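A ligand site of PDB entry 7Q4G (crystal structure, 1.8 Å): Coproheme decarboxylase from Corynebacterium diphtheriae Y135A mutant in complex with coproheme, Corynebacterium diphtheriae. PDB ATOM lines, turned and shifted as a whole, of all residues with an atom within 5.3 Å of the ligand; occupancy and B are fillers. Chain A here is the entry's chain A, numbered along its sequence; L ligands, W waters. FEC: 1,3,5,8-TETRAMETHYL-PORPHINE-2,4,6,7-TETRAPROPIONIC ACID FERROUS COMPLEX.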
ATOM      1  N   ALA A 114       8.948 -26.093 -35.197  1.00  0.00           N
ATOM      2  CA  ALA A 114       8.049 -27.160 -34.792  1.00  0.00           C
ATOM      3  C   ALA A 114       7.879 -28.156 -35.942  1.00  0.00           C
ATOM      4  O   ALA A 114       8.043 -27.820 -37.121  1.00  0.00           O
ATOM      5  CB  ALA A 114       6.690 -26.630 -34.368  1.00  0.00           C
ATOM      6  N   ASN A 117       3.430 -27.405 -36.954  1.00  0.00           N
ATOM      7  CA  ASN A 117       2.890 -26.046 -36.965  1.00  0.00           C
ATOM      8  C   ASN A 117       4.012 -25.033 -36.855  1.00  0.00           C
ATOM      9  O   ASN A 117       4.460 -24.698 -35.739  1.00  0.00           O
ATOM     10  CB  ASN A 117       1.905 -25.834 -35.809  1.00  0.00           C
ATOM     11  CG  ASN A 117       1.242 -24.460 -35.878  1.00  0.00           C
ATOM     12  OD1 ASN A 117       1.528 -23.672 -36.764  1.00  0.00           O
ATOM     13  ND2 ASN A 117       0.340 -24.211 -34.962  1.00  0.00           N
ATOM     14  N   HIS A 120       4.087 -21.950 -34.566  1.00  0.00           N
ATOM     15  CA  HIS A 120       4.338 -22.131 -33.150  1.00  0.00           C
ATOM     16  C   HIS A 120       5.808 -21.864 -32.897  1.00  0.00           C
ATOM     17  O   HIS A 120       6.660 -22.662 -33.293  1.00  0.00           O
ATOM     18  CB  HIS A 120       3.969 -23.560 -32.720  1.00  0.00           C
ATOM     19  CG  HIS A 120       4.383 -23.912 -31.319  1.00  0.00           C
ATOM     20  ND1 HIS A 120       3.696 -23.486 -30.208  1.00  0.00           N
ATOM     21  CD2 HIS A 120       5.437 -24.643 -30.868  1.00  0.00           C
ATOM     22  CE1 HIS A 120       4.294 -23.967 -29.125  1.00  0.00           C
ATOM     23  NE2 HIS A 120       5.375 -24.629 -29.494  1.00  0.00           N
ATOM     24  N   LEU A 121       6.100 -20.770 -32.212  1.00  0.00           N
ATOM     25  CA  LEU A 121       7.470 -20.326 -31.985  1.00  0.00           C
ATOM     26  C   LEU A 121       7.618 -19.873 -30.539  1.00  0.00           C
ATOM     27  O   LEU A 121       6.673 -19.294 -29.983  1.00  0.00           O
ATOM     28  CB  LEU A 121       7.852 -19.162 -32.919  1.00  0.00           C
ATOM     29  CG  LEU A 121       7.956 -19.501 -34.419  1.00  0.00           C
ATOM     30  CD1 LEU A 121       7.516 -18.292 -35.210  1.00  0.00           C
ATOM     31  CD2 LEU A 121       9.338 -19.863 -34.849  1.00  0.00           C
ATOM     32  N   PHE A 139      11.287 -31.747 -20.250  1.00  0.00           N
ATOM     33  CA  PHE A 139      10.281 -32.683 -20.691  1.00  0.00           C
ATOM     34  C   PHE A 139      10.936 -33.834 -21.416  1.00  0.00           C
ATOM     35  O   PHE A 139      11.882 -33.630 -22.186  1.00  0.00           O
ATOM     36  CB  PHE A 139       9.254 -31.994 -21.610  1.00  0.00           C
ATOM     37  CG  PHE A 139       7.874 -32.596 -21.555  1.00  0.00           C
ATOM     38  CD1 PHE A 139       7.521 -33.636 -22.405  1.00  0.00           C
ATOM     39  CD2 PHE A 139       6.934 -32.118 -20.676  1.00  0.00           C
ATOM     40  CE1 PHE A 139       6.242 -34.179 -22.372  1.00  0.00           C
ATOM     41  CE2 PHE A 139       5.630 -32.670 -20.650  1.00  0.00           C
ATOM     42  CZ  PHE A 139       5.306 -33.730 -21.495  1.00  0.00           C
ATOM     43  N   ARG A 141       9.275 -37.165 -23.590  1.00  0.00           N
ATOM     44  CA  ARG A 141       8.142 -37.908 -24.123  1.00  0.00           C
ATOM     45  C   ARG A 141       8.326 -39.430 -23.982  1.00  0.00           C
ATOM     46  O   ARG A 141       9.439 -39.968 -23.783  1.00  0.00           O
ATOM     47  CB  ARG A 141       7.980 -37.532 -25.623  1.00  0.00           C
ATOM     48  CG  ARG A 141       7.418 -36.193 -25.864  1.00  0.00           C
ATOM     49  CD  ARG A 141       5.892 -36.186 -25.727  1.00  0.00           C
ATOM     50  NE  ARG A 141       5.353 -34.876 -25.872  1.00  0.00           N
ATOM     51  CZ  ARG A 141       4.202 -34.451 -25.292  1.00  0.00           C
ATOM     52  NH1 ARG A 141       3.510 -35.222 -24.488  1.00  0.00           N
ATOM     53  NH2 ARG A 141       3.800 -33.207 -25.502  1.00  0.00           N
ATOM     54  N   TRP A 145       6.490 -41.899 -28.853  1.00  0.00           N
ATOM     55  CA  TRP A 145       5.913 -40.642 -29.327  1.00  0.00           C
ATOM     56  C   TRP A 145       6.339 -40.325 -30.749  1.00  0.00           C
ATOM     57  O   TRP A 145       5.520 -39.926 -31.595  1.00  0.00           O
ATOM     58  CB  TRP A 145       6.290 -39.530 -28.380  1.00  0.00           C
ATOM     59  CG  TRP A 145       5.859 -38.137 -28.750  1.00  0.00           C
ATOM     60  CD1 TRP A 145       6.670 -37.076 -29.054  1.00  0.00           C
ATOM     61  CD2 TRP A 145       4.546 -37.629 -28.747  1.00  0.00           C
ATOM     62  NE1 TRP A 145       5.968 -35.954 -29.255  1.00  0.00           N
ATOM     63  CE2 TRP A 145       4.630 -36.254 -29.061  1.00  0.00           C
ATOM     64  CE3 TRP A 145       3.280 -38.201 -28.519  1.00  0.00           C
ATOM     65  CZ2 TRP A 145       3.492 -35.470 -29.198  1.00  0.00           C
ATOM     66  CZ3 TRP A 145       2.172 -37.413 -28.629  1.00  0.00           C
ATOM     67  CH2 TRP A 145       2.267 -36.055 -28.931  1.00  0.00           C
ATOM     68  N   TYR A 146       7.635 -40.411 -31.023  1.00  0.00           N
ATOM     69  CA  TYR A 146       8.134 -39.893 -32.311  1.00  0.00           C
ATOM     70  C   TYR A 146       7.939 -40.870 -33.453  1.00  0.00           C
ATOM     71  O   TYR A 146       7.918 -40.438 -34.603  1.00  0.00           O
ATOM     72  CB  TYR A 146       9.587 -39.499 -32.198  1.00  0.00           C
ATOM     73  CG  TYR A 146       9.880 -38.547 -31.035  1.00  0.00           C
ATOM     74  CD1 TYR A 146       9.772 -37.186 -31.201  1.00  0.00           C
ATOM     75  CD2 TYR A 146      10.245 -39.047 -29.762  1.00  0.00           C
ATOM     76  CE1 TYR A 146      10.055 -36.326 -30.184  1.00  0.00           C
ATOM     77  CE2 TYR A 146      10.558 -38.208 -28.769  1.00  0.00           C
ATOM     78  CZ  TYR A 146      10.439 -36.818 -28.990  1.00  0.00           C
ATOM     79  OH  TYR A 146      10.699 -35.926 -27.995  1.00  0.00           O
ATOM     80  N   ARG A 153       0.170 -38.032 -34.360  1.00  0.00           N
ATOM     81  CA  ARG A 153       0.893 -37.098 -33.484  1.00  0.00           C
ATOM     82  C   ARG A 153       0.485 -35.656 -33.779  1.00  0.00           C
ATOM     83  O   ARG A 153       0.330 -34.846 -32.864  1.00  0.00           O
ATOM     84  CB  ARG A 153       2.422 -37.254 -33.683  1.00  0.00           C
ATOM     85  CG  ARG A 153       3.237 -36.344 -32.770  1.00  0.00           C
ATOM     86  CD  ARG A 153       4.808 -36.644 -32.805  1.00  0.00           C
ATOM     87  NE  ARG A 153       5.307 -36.764 -34.144  1.00  0.00           N
ATOM     88  CZ  ARG A 153       5.368 -37.898 -34.833  1.00  0.00           C
ATOM     89  NH1 ARG A 153       4.982 -39.052 -34.298  1.00  0.00           N
ATOM     90  NH2 ARG A 153       5.831 -37.862 -36.085  1.00  0.00           N
ATOM     91  N   LEU A 157      -1.100 -33.127 -30.992  1.00  0.00           N
ATOM     92  CA  LEU A 157      -0.575 -31.808 -30.673  1.00  0.00           C
ATOM     93  C   LEU A 157      -1.564 -30.666 -31.022  1.00  0.00           C
ATOM     94  O   LEU A 157      -1.575 -29.630 -30.378  1.00  0.00           O
ATOM     95  CB  LEU A 157       0.753 -31.561 -31.412  1.00  0.00           C
ATOM     96  CG  LEU A 157       1.987 -32.271 -30.845  1.00  0.00           C
ATOM     97  CD1 LEU A 157       3.199 -32.181 -31.853  1.00  0.00           C
ATOM     98  CD2 LEU A 157       2.409 -31.647 -29.525  1.00  0.00           C
ATOM     99  N   ALA A 158      -2.353 -30.831 -32.076  1.00  0.00           N
ATOM    100  CA  ALA A 158      -3.361 -29.798 -32.375  1.00  0.00           C
ATOM    101  C   ALA A 158      -4.391 -29.722 -31.236  1.00  0.00           C
ATOM    102  O   ALA A 158      -4.791 -28.629 -30.820  1.00  0.00           O
ATOM    103  CB  ALA A 158      -4.022 -30.087 -33.692  1.00  0.00           C
ATOM    104  N   HIS A 160      -3.818 -30.642 -28.145  1.00  0.00           N
ATOM    105  CA  HIS A 160      -3.052 -30.075 -27.058  1.00  0.00           C
ATOM    106  C   HIS A 160      -3.046 -28.565 -27.132  1.00  0.00           C
ATOM    107  O   HIS A 160      -3.345 -27.875 -26.152  1.00  0.00           O
ATOM    108  CB  HIS A 160      -1.631 -30.707 -27.110  1.00  0.00           C
ATOM    109  CG  HIS A 160      -0.547 -29.969 -26.422  1.00  0.00           C
ATOM    110  ND1 HIS A 160      -0.087 -30.329 -25.176  1.00  0.00           N
ATOM    111  CD2 HIS A 160       0.257 -28.970 -26.843  1.00  0.00           C
ATOM    112  CE1 HIS A 160       0.931 -29.537 -24.837  1.00  0.00           C
ATOM    113  NE2 HIS A 160       1.160 -28.707 -25.831  1.00  0.00           N
ATOM    114  N   GLY A 161      -2.777 -27.998 -28.333  1.00  0.00           N
ATOM    115  CA  GLY A 161      -2.783 -26.561 -28.463  1.00  0.00           C
ATOM    116  C   GLY A 161      -4.165 -25.984 -28.216  1.00  0.00           C
ATOM    117  O   GLY A 161      -4.300 -24.919 -27.615  1.00  0.00           O
ATOM    118  N   ALA A 164      -5.272 -25.083 -24.647  1.00  0.00           N
ATOM    119  CA  ALA A 164      -4.718 -23.871 -24.057  1.00  0.00           C
ATOM    120  C   ALA A 164      -5.305 -22.616 -24.632  1.00  0.00           C
ATOM    121  O   ALA A 164      -4.795 -21.519 -24.347  1.00  0.00           O
ATOM    122  CB  ALA A 164      -3.190 -23.852 -24.238  1.00  0.00           C
ATOM    123  N   PHE A 167      -5.902 -19.409 -22.629  1.00  0.00           N
ATOM    124  CA  PHE A 167      -4.773 -18.886 -21.891  1.00  0.00           C
ATOM    125  C   PHE A 167      -3.813 -18.144 -22.807  1.00  0.00           C
ATOM    126  O   PHE A 167      -2.592 -18.378 -22.741  1.00  0.00           O
ATOM    127  CB  PHE A 167      -4.046 -20.032 -21.180  1.00  0.00           C
ATOM    128  CG  PHE A 167      -4.888 -20.733 -20.152  1.00  0.00           C
ATOM    129  CD1 PHE A 167      -5.690 -21.828 -20.517  1.00  0.00           C
ATOM    130  CD2 PHE A 167      -4.894 -20.315 -18.836  1.00  0.00           C
ATOM    131  CE1 PHE A 167      -6.470 -22.481 -19.559  1.00  0.00           C
ATOM    132  CE2 PHE A 167      -5.693 -20.956 -17.879  1.00  0.00           C
ATOM    133  CZ  PHE A 167      -6.467 -22.057 -18.253  1.00  0.00           C
ATOM    134  N   VAL A 170      -0.612 -16.612 -21.200  1.00  0.00           N
ATOM    135  CA  VAL A 170       0.517 -17.423 -20.765  1.00  0.00           C
ATOM    136  C   VAL A 170       1.293 -17.772 -22.021  1.00  0.00           C
ATOM    137  O   VAL A 170       0.820 -18.559 -22.876  1.00  0.00           O
ATOM    138  CB  VAL A 170       0.067 -18.677 -20.026  1.00  0.00           C
ATOM    139  CG1 VAL A 170       1.261 -19.436 -19.448  1.00  0.00           C
ATOM    140  CG2 VAL A 170      -0.981 -18.325 -18.923  1.00  0.00           C
ATOM    141  N   ALA A 172       4.197 -19.495 -24.162  1.00  0.00           N
ATOM    142  CA  ALA A 172       4.943 -20.748 -24.110  1.00  0.00           C
ATOM    143  C   ALA A 172       6.283 -20.631 -24.794  1.00  0.00           C
ATOM    144  O   ALA A 172       6.430 -19.870 -25.764  1.00  0.00           O
ATOM    145  CB  ALA A 172       4.085 -21.827 -24.805  1.00  0.00           C
ATOM    146  N   THR A 174       8.686 -23.805 -26.020  1.00  0.00           N
ATOM    147  CA  THR A 174       8.995 -25.233 -26.124  1.00  0.00           C
ATOM    148  C   THR A 174      10.180 -25.395 -27.082  1.00  0.00           C
ATOM    149  O   THR A 174      10.086 -24.987 -28.247  1.00  0.00           O
ATOM    150  CB  THR A 174       7.749 -25.993 -26.563  1.00  0.00           C
ATOM    151  OG1 THR A 174       7.469 -25.740 -27.946  1.00  0.00           O
ATOM    152  CG2 THR A 174       6.544 -25.552 -25.721  1.00  0.00           C
ATOM    153  N   TRP A 185      13.149 -31.797 -24.197  1.00  0.00           N
ATOM    154  CA  TRP A 185      12.678 -30.410 -24.415  1.00  0.00           C
ATOM    155  C   TRP A 185      12.932 -29.590 -23.152  1.00  0.00           C
ATOM    156  O   TRP A 185      13.035 -30.126 -22.043  1.00  0.00           O
ATOM    157  CB  TRP A 185      11.152 -30.439 -24.737  1.00  0.00           C
ATOM    158  CG  TRP A 185      10.824 -31.268 -25.888  1.00  0.00           C
ATOM    159  CD1 TRP A 185      10.610 -32.625 -25.867  1.00  0.00           C
ATOM    160  CD2 TRP A 185      10.744 -30.857 -27.250  1.00  0.00           C
ATOM    161  NE1 TRP A 185      10.365 -33.065 -27.151  1.00  0.00           N
ATOM    162  CE2 TRP A 185      10.454 -32.021 -28.017  1.00  0.00           C
ATOM    163  CE3 TRP A 185      10.898 -29.630 -27.928  1.00  0.00           C
ATOM    164  CZ2 TRP A 185      10.317 -31.990 -29.410  1.00  0.00           C
ATOM    165  CZ3 TRP A 185      10.722 -29.582 -29.286  1.00  0.00           C
ATOM    166  CH2 TRP A 185      10.431 -30.744 -30.023  1.00  0.00           C
ATOM    167  N   LEU A 187      11.038 -26.370 -21.313  1.00  0.00           N
ATOM    168  CA  LEU A 187       9.765 -25.652 -21.290  1.00  0.00           C
ATOM    169  C   LEU A 187       9.872 -24.390 -20.421  1.00  0.00           C
ATOM    170  O   LEU A 187      10.461 -24.395 -19.345  1.00  0.00           O
ATOM    171  CB  LEU A 187       8.635 -26.497 -20.782  1.00  0.00           C
ATOM    172  CG  LEU A 187       8.363 -27.800 -21.534  1.00  0.00           C
ATOM    173  CD1 LEU A 187       7.181 -28.555 -20.875  1.00  0.00           C
ATOM    174  CD2 LEU A 187       8.054 -27.615 -22.968  1.00  0.00           C
ATOM    175  N   PHE A 189       7.041 -21.154 -19.344  1.00  0.00           N
ATOM    176  CA  PHE A 189       5.713 -20.548 -19.454  1.00  0.00           C
ATOM    177  C   PHE A 189       5.742 -19.260 -18.649  1.00  0.00           C
ATOM    178  O   PHE A 189       6.084 -19.262 -17.475  1.00  0.00           O
ATOM    179  CB  PHE A 189       4.651 -21.523 -18.983  1.00  0.00           C
ATOM    180  CG  PHE A 189       4.680 -22.836 -19.761  1.00  0.00           C
ATOM    181  CD1 PHE A 189       4.268 -22.863 -21.070  1.00  0.00           C
ATOM    182  CD2 PHE A 189       5.188 -23.973 -19.175  1.00  0.00           C
ATOM    183  CE1 PHE A 189       4.355 -24.048 -21.812  1.00  0.00           C
ATOM    184  CE2 PHE A 189       5.282 -25.145 -19.905  1.00  0.00           C
ATOM    185  CZ  PHE A 189       4.885 -25.176 -21.233  1.00  0.00           C
ATOM    186  N   LEU A 200      -3.395 -23.114 -16.273  1.00  0.00           N
ATOM    187  CA  LEU A 200      -3.053 -23.684 -17.575  1.00  0.00           C
ATOM    188  C   LEU A 200      -2.571 -25.112 -17.429  1.00  0.00           C
ATOM    189  O   LEU A 200      -2.977 -26.008 -18.202  1.00  0.00           O
ATOM    190  CB  LEU A 200      -2.001 -22.826 -18.274  1.00  0.00           C
ATOM    191  CG  LEU A 200      -1.414 -23.486 -19.550  1.00  0.00           C
ATOM    192  CD1 LEU A 200      -2.511 -23.593 -20.641  1.00  0.00           C
ATOM    193  CD2 LEU A 200      -0.204 -22.807 -20.033  1.00  0.00           C
ATOM    194  N   MET A 201      -1.645 -25.347 -16.488  1.00  0.00           N
ATOM    195  CA  MET A 201      -1.110 -26.728 -16.343  1.00  0.00           C
ATOM    196  C   MET A 201      -2.182 -27.705 -15.972  1.00  0.00           C
ATOM    197  O   MET A 201      -2.209 -28.823 -16.509  1.00  0.00           O
ATOM    198  CB  MET A 201      -0.025 -26.727 -15.256  1.00  0.00           C
ATOM    199  CG  MET A 201       1.197 -25.966 -15.616  1.00  0.00           C
ATOM    200  SD  MET A 201       2.307 -26.939 -16.649  1.00  0.00           S
ATOM    201  CE  MET A 201       3.746 -25.913 -16.489  1.00  0.00           C
ATOM    202  N   MET A 204      -4.243 -28.465 -19.075  1.00  0.00           N
ATOM    203  CA  MET A 204      -3.549 -29.205 -20.088  1.00  0.00           C
ATOM    204  C   MET A 204      -3.432 -30.681 -19.712  1.00  0.00           C
ATOM    205  O   MET A 204      -3.061 -31.466 -20.567  1.00  0.00           O
ATOM    206  CB  MET A 204      -2.146 -28.609 -20.306  1.00  0.00           C
ATOM    207  CG  MET A 204      -2.183 -27.187 -20.871  1.00  0.00           C
ATOM    208  SD  MET A 204      -2.863 -27.229 -22.519  1.00  0.00           S
ATOM    209  CE  MET A 204      -1.400 -27.760 -23.434  1.00  0.00           C
ATOM    210  N   ARG A 205      -3.747 -31.085 -18.458  1.00  0.00           N
ATOM    211  CA  ARG A 205      -3.814 -32.491 -18.135  1.00  0.00           C
ATOM    212  C   ARG A 205      -4.950 -33.194 -18.880  1.00  0.00           C
ATOM    213  O   ARG A 205      -4.972 -34.436 -19.006  1.00  0.00           O
ATOM    214  CB  ARG A 205      -4.012 -32.638 -16.610  1.00  0.00           C
ATOM    215  CG  ARG A 205      -2.796 -32.279 -15.789  1.00  0.00           C
ATOM    216  CD  ARG A 205      -1.673 -33.311 -16.050  1.00  0.00           C
ATOM    217  NE  ARG A 205      -0.633 -33.298 -15.045  1.00  0.00           N
ATOM    218  CZ  ARG A 205       0.448 -32.505 -15.022  1.00  0.00           C
ATOM    219  NH1 ARG A 205       0.642 -31.600 -15.937  1.00  0.00           N
ATOM    220  NH2 ARG A 205       1.370 -32.681 -14.064  1.00  0.00           N
ATOM    221  N   THR A 207      -5.735 -33.831 -21.909  1.00  0.00           N
ATOM    222  CA  THR A 207      -5.399 -34.029 -23.309  1.00  0.00           C
ATOM    223  C   THR A 207      -4.821 -35.415 -23.539  1.00  0.00           C
ATOM    224  O   THR A 207      -4.148 -35.980 -22.672  1.00  0.00           O
ATOM    225  CB  THR A 207      -4.387 -33.010 -23.801  1.00  0.00           C
ATOM    226  OG1 THR A 207      -3.199 -33.122 -22.992  1.00  0.00           O
ATOM    227  CG2 THR A 207      -4.948 -31.554 -23.701  1.00  0.00           C
ATOM    228  N   ARG A 210      -1.131 -36.509 -22.815  1.00  0.00           N
ATOM    229  CA  ARG A 210      -0.679 -36.928 -21.486  1.00  0.00           C
ATOM    230  C   ARG A 210      -0.386 -38.411 -21.430  1.00  0.00           C
ATOM    231  O   ARG A 210       0.311 -38.861 -20.496  1.00  0.00           O
ATOM    232  CB  ARG A 210      -1.756 -36.618 -20.449  1.00  0.00           C
ATOM    233  CG  ARG A 210      -1.925 -35.098 -20.128  1.00  0.00           C
ATOM    234  CD  ARG A 210      -0.634 -34.452 -19.778  1.00  0.00           C
ATOM    235  NE  ARG A 210      -0.062 -34.950 -18.525  1.00  0.00           N
ATOM    236  CZ  ARG A 210       1.145 -34.614 -18.064  1.00  0.00           C
ATOM    237  NH1 ARG A 210       1.880 -33.674 -18.635  1.00  0.00           N
ATOM    238  NH2 ARG A 210       1.604 -35.212 -16.969  1.00  0.00           N
ATOM    239  N   GLU A 216       8.969 -34.941 -16.472  1.00  0.00           N
ATOM    240  CA  GLU A 216       8.615 -33.530 -16.607  1.00  0.00           C
ATOM    241  C   GLU A 216       9.045 -32.704 -15.398  1.00  0.00           C
ATOM    242  O   GLU A 216       8.641 -31.552 -15.276  1.00  0.00           O
ATOM    243  CB  GLU A 216       7.119 -33.408 -16.966  1.00  0.00           C
ATOM    244  CG  GLU A 216       6.145 -33.528 -15.928  1.00  0.00           C
ATOM    245  CD  GLU A 216       4.724 -33.968 -16.428  1.00  0.00           C
ATOM    246  OE1 GLU A 216       4.085 -33.180 -17.162  1.00  0.00           O
ATOM    247  OE2 GLU A 216       4.163 -35.060 -16.053  1.00  0.00           O
HETATM  248  O1A FEC L   1       6.543 -32.821 -27.348  1.00  0.00           O
HETATM  249  CGA FEC L   1       6.612 -32.505 -28.579  1.00  0.00           C
HETATM  250  O2A FEC L   1       6.822 -33.319 -29.489  1.00  0.00           O
HETATM  251  CBA FEC L   1       6.805 -31.030 -28.748  1.00  0.00           C
HETATM  252  CAA FEC L   1       7.242 -30.331 -27.469  1.00  0.00           C
HETATM  253  C3A FEC L   1       6.105 -29.848 -26.536  1.00  0.00           C
HETATM  254  C2A FEC L   1       5.904 -30.206 -25.221  1.00  0.00           C
HETATM  255  C1A FEC L   1       4.768 -29.385 -24.758  1.00  0.00           C
HETATM  256  CHA FEC L   1       4.130 -29.396 -23.534  1.00  0.00           C
HETATM  257  C4D FEC L   1       3.432 -28.301 -23.085  1.00  0.00           C
HETATM  258  ND  FEC L   1       2.867 -27.290 -23.832  1.00  0.00           N
HETATM  259  C1D FEC L   1       2.205 -26.383 -22.967  1.00  0.00           C
HETATM  260  CHD FEC L   1       1.585 -25.195 -23.392  1.00  0.00           C
HETATM  261  C4C FEC L   1       1.234 -24.983 -24.739  1.00  0.00           C
HETATM  262  C3C FEC L   1       0.363 -23.910 -25.140  1.00  0.00           C
HETATM  263  C2C FEC L   1       0.166 -24.046 -26.509  1.00  0.00           C
HETATM  264  C1C FEC L   1       0.921 -25.195 -26.946  1.00  0.00           C
HETATM  265  CHC FEC L   1       0.991 -25.733 -28.217  1.00  0.00           C
HETATM  266  C4B FEC L   1       2.108 -26.452 -28.605  1.00  0.00           C
HETATM  267  C3B FEC L   1       2.488 -26.549 -29.966  1.00  0.00           C
HETATM  268  C2B FEC L   1       3.660 -27.315 -30.040  1.00  0.00           C
HETATM  269  C1B FEC L   1       3.958 -27.637 -28.655  1.00  0.00           C
HETATM  270  NB  FEC L   1       2.980 -27.109 -27.793  1.00  0.00           N
HETATM  271 FE   FEC L   1       2.796 -27.294 -25.815  1.00  0.00          FE
HETATM  272  NA  FEC L   1       4.276 -28.621 -25.827  1.00  0.00           N
HETATM  273  C4A FEC L   1       5.135 -28.818 -26.885  1.00  0.00           C
HETATM  274  CHB FEC L   1       5.071 -28.335 -28.177  1.00  0.00           C
HETATM  275  NC  FEC L   1       1.545 -25.746 -25.835  1.00  0.00           N
HETATM  276  CMB FEC L   1       4.560 -27.716 -31.275  1.00  0.00           C
HETATM  277  CAB FEC L   1       1.724 -25.995 -31.116  1.00  0.00           C
HETATM  278  CBB FEC L   1       0.561 -26.959 -31.427  1.00  0.00           C
HETATM  279  CGB FEC L   1      -0.367 -26.473 -32.542  1.00  0.00           C
HETATM  280  O1B FEC L   1      -0.530 -27.146 -33.543  1.00  0.00           O
HETATM  281  O2B FEC L   1      -1.208 -25.548 -32.162  1.00  0.00           O
HETATM  282  CAC FEC L   1      -0.702 -23.200 -27.401  1.00  0.00           C
HETATM  283  CBC FEC L   1      -0.067 -21.837 -27.685  1.00  0.00           C
HETATM  284  CGC FEC L   1       1.246 -21.907 -28.467  1.00  0.00           C
HETATM  285  O1C FEC L   1       2.281 -21.426 -28.070  1.00  0.00           O
HETATM  286  O2C FEC L   1       1.140 -22.428 -29.661  1.00  0.00           O
HETATM  287  CMC FEC L   1      -0.275 -22.802 -24.192  1.00  0.00           C
HETATM  288  C2D FEC L   1       2.414 -26.855 -21.594  1.00  0.00           C
HETATM  289  C3D FEC L   1       3.113 -28.063 -21.689  1.00  0.00           C
HETATM  290  CAD FEC L   1       3.532 -28.910 -20.525  1.00  0.00           C
HETATM  291  CBD FEC L   1       2.355 -29.600 -19.860  1.00  0.00           C
HETATM  292  CGD FEC L   1       1.823 -30.810 -20.620  1.00  0.00           C
HETATM  293  O1D FEC L   1       0.674 -31.140 -20.588  1.00  0.00           O
HETATM  294  O2D FEC L   1       2.606 -31.211 -21.576  1.00  0.00           O
HETATM  295  CMD FEC L   1       1.866 -26.158 -20.286  1.00  0.00           C
HETATM  296  CMA FEC L   1       6.755 -31.247 -24.392  1.00  0.00           C
HETATM  297  O   HOH W   1      -2.230 -26.966 -35.740  1.00  0.00           O
HETATM  298  O   HOH W   2      -0.655 -30.838 -18.053  1.00  0.00           O
HETATM  299  O   HOH W   3       1.763 -33.323 -23.278  1.00  0.00           O
HETATM  300  O   HOH W   4      -0.267 -30.226 -35.019  1.00  0.00           O
HETATM  301  O   HOH W   5      -0.664 -32.027 -22.961  1.00  0.00           O
HETATM  302  O   HOH W   6      -4.065 -26.297 -32.157  1.00  0.00           O
HETATM  303  O   HOH W   7       5.210 -21.076 -28.435  1.00  0.00           O
HETATM  304  O   HOH W   8      -1.219 -23.168 -30.742  1.00  0.00           O
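An iron atom (FE) of the ligand is bound by a ring nitrogen (NE2) of His 160 (2.2 Å). An oxygen (O2A) of the ligand sits at hydrogen-bond distance from the indole nitrogen of Trp 145. The guanidinium group (NE) of Arg 141 lies within salt-bridge range of an oxygen (O1A) of the ligand, at 2.8 Å. An oxygen (O2C) of the ligand lies within hydrogen-bond range of a ring nitrogen (ND1) of His 120, 2.8 Å away. The side-chain amide nitrogen (ND2) of Asn 117 sits at hydrogen-bond distance from an oxygen (O1B) of the ligand (3.4 Å). NH1 of Arg 210 is in salt-bridge range of O1D of the ligand.
O of Trp 145 lies within hydrogen-bond range of NH1 of Arg 153. A ring nitrogen (NE2) of His 120 lies within hydrogen-bond range of the side-chain hydroxyl (OG1) of Thr 174, 2.8 Å away. N of Phe 139 lies within hydrogen-bond range of O of Trp 185. The side-chain carboxylate of Glu 216 lies within salt-bridge range of the guanidinium group of Arg 210 (2.7 Å). The side-chain hydroxyl (OH) of Tyr 146 lies within hydrogen-bond range of the indole nitrogen (NE1) of Trp 185. The backbone carbonyl oxygen (O) of Met 204 is in hydrogen-bond range of the side-chain hydroxyl (OG1) of Thr 207 (2.9 Å).
Merely in contact with the ligand: Phe 189, Ala 164, Phe 139, Thr 174, Trp 185, Leu 157, Leu 187, Met 201, Met 204, Ala 172, Gly 161, Ala 114 and Leu 200. Hydrophobic or aromatic side chains within 4 Å of the ligand: Ala 114, His 120, Phe 139, Trp 145, His 160, Ala 164, Ala 172, Trp 185, Leu 187, Phe 189, Leu 200, Met 201 and Met 204. 19 residues have an atom within 4 Å of the ligand: Ala 114, Asn 117, His 120, Phe 139, Arg 141, Trp 145, Leu 157, His 160, Gly 161, Ala 164, Ala 172, Thr 174, Trp 185, Leu 187, Phe 189, Leu 200, Met 201, Met 204 and Arg 210. The nearest printed residue that does not touch the ligand is Ala 158 (4.1 Å).
Water W3 bridges an oxygen (O2D) of the ligand and the guanidinium group (NH1) of Arg 141. Water W5 lies within hydrogen-bond range of OG1 of Thr 207 (2.8 Å), ND1 of His 160 (2.8 Å), O1D of the ligand (2.9 Å) and O of Met 204 (3.4 Å). Water W2 lies within hydrogen-bond range of NH1 of Arg 205 (2.6 Å), O1D of the ligand (2.9 Å) and O of Met 201 (3.0 Å). Water W6 bridges O of Ala 158 (2.8 Å) and O2B of the ligand (3.0 Å). Water W7 lies within hydrogen-bond range of the backbone carbonyl oxygen (O) of Leu 121, an oxygen (O1C) of the ligand, the backbone carbonyl oxygen (O) of Ala 172 and a ring nitrogen (ND1) of His 120.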
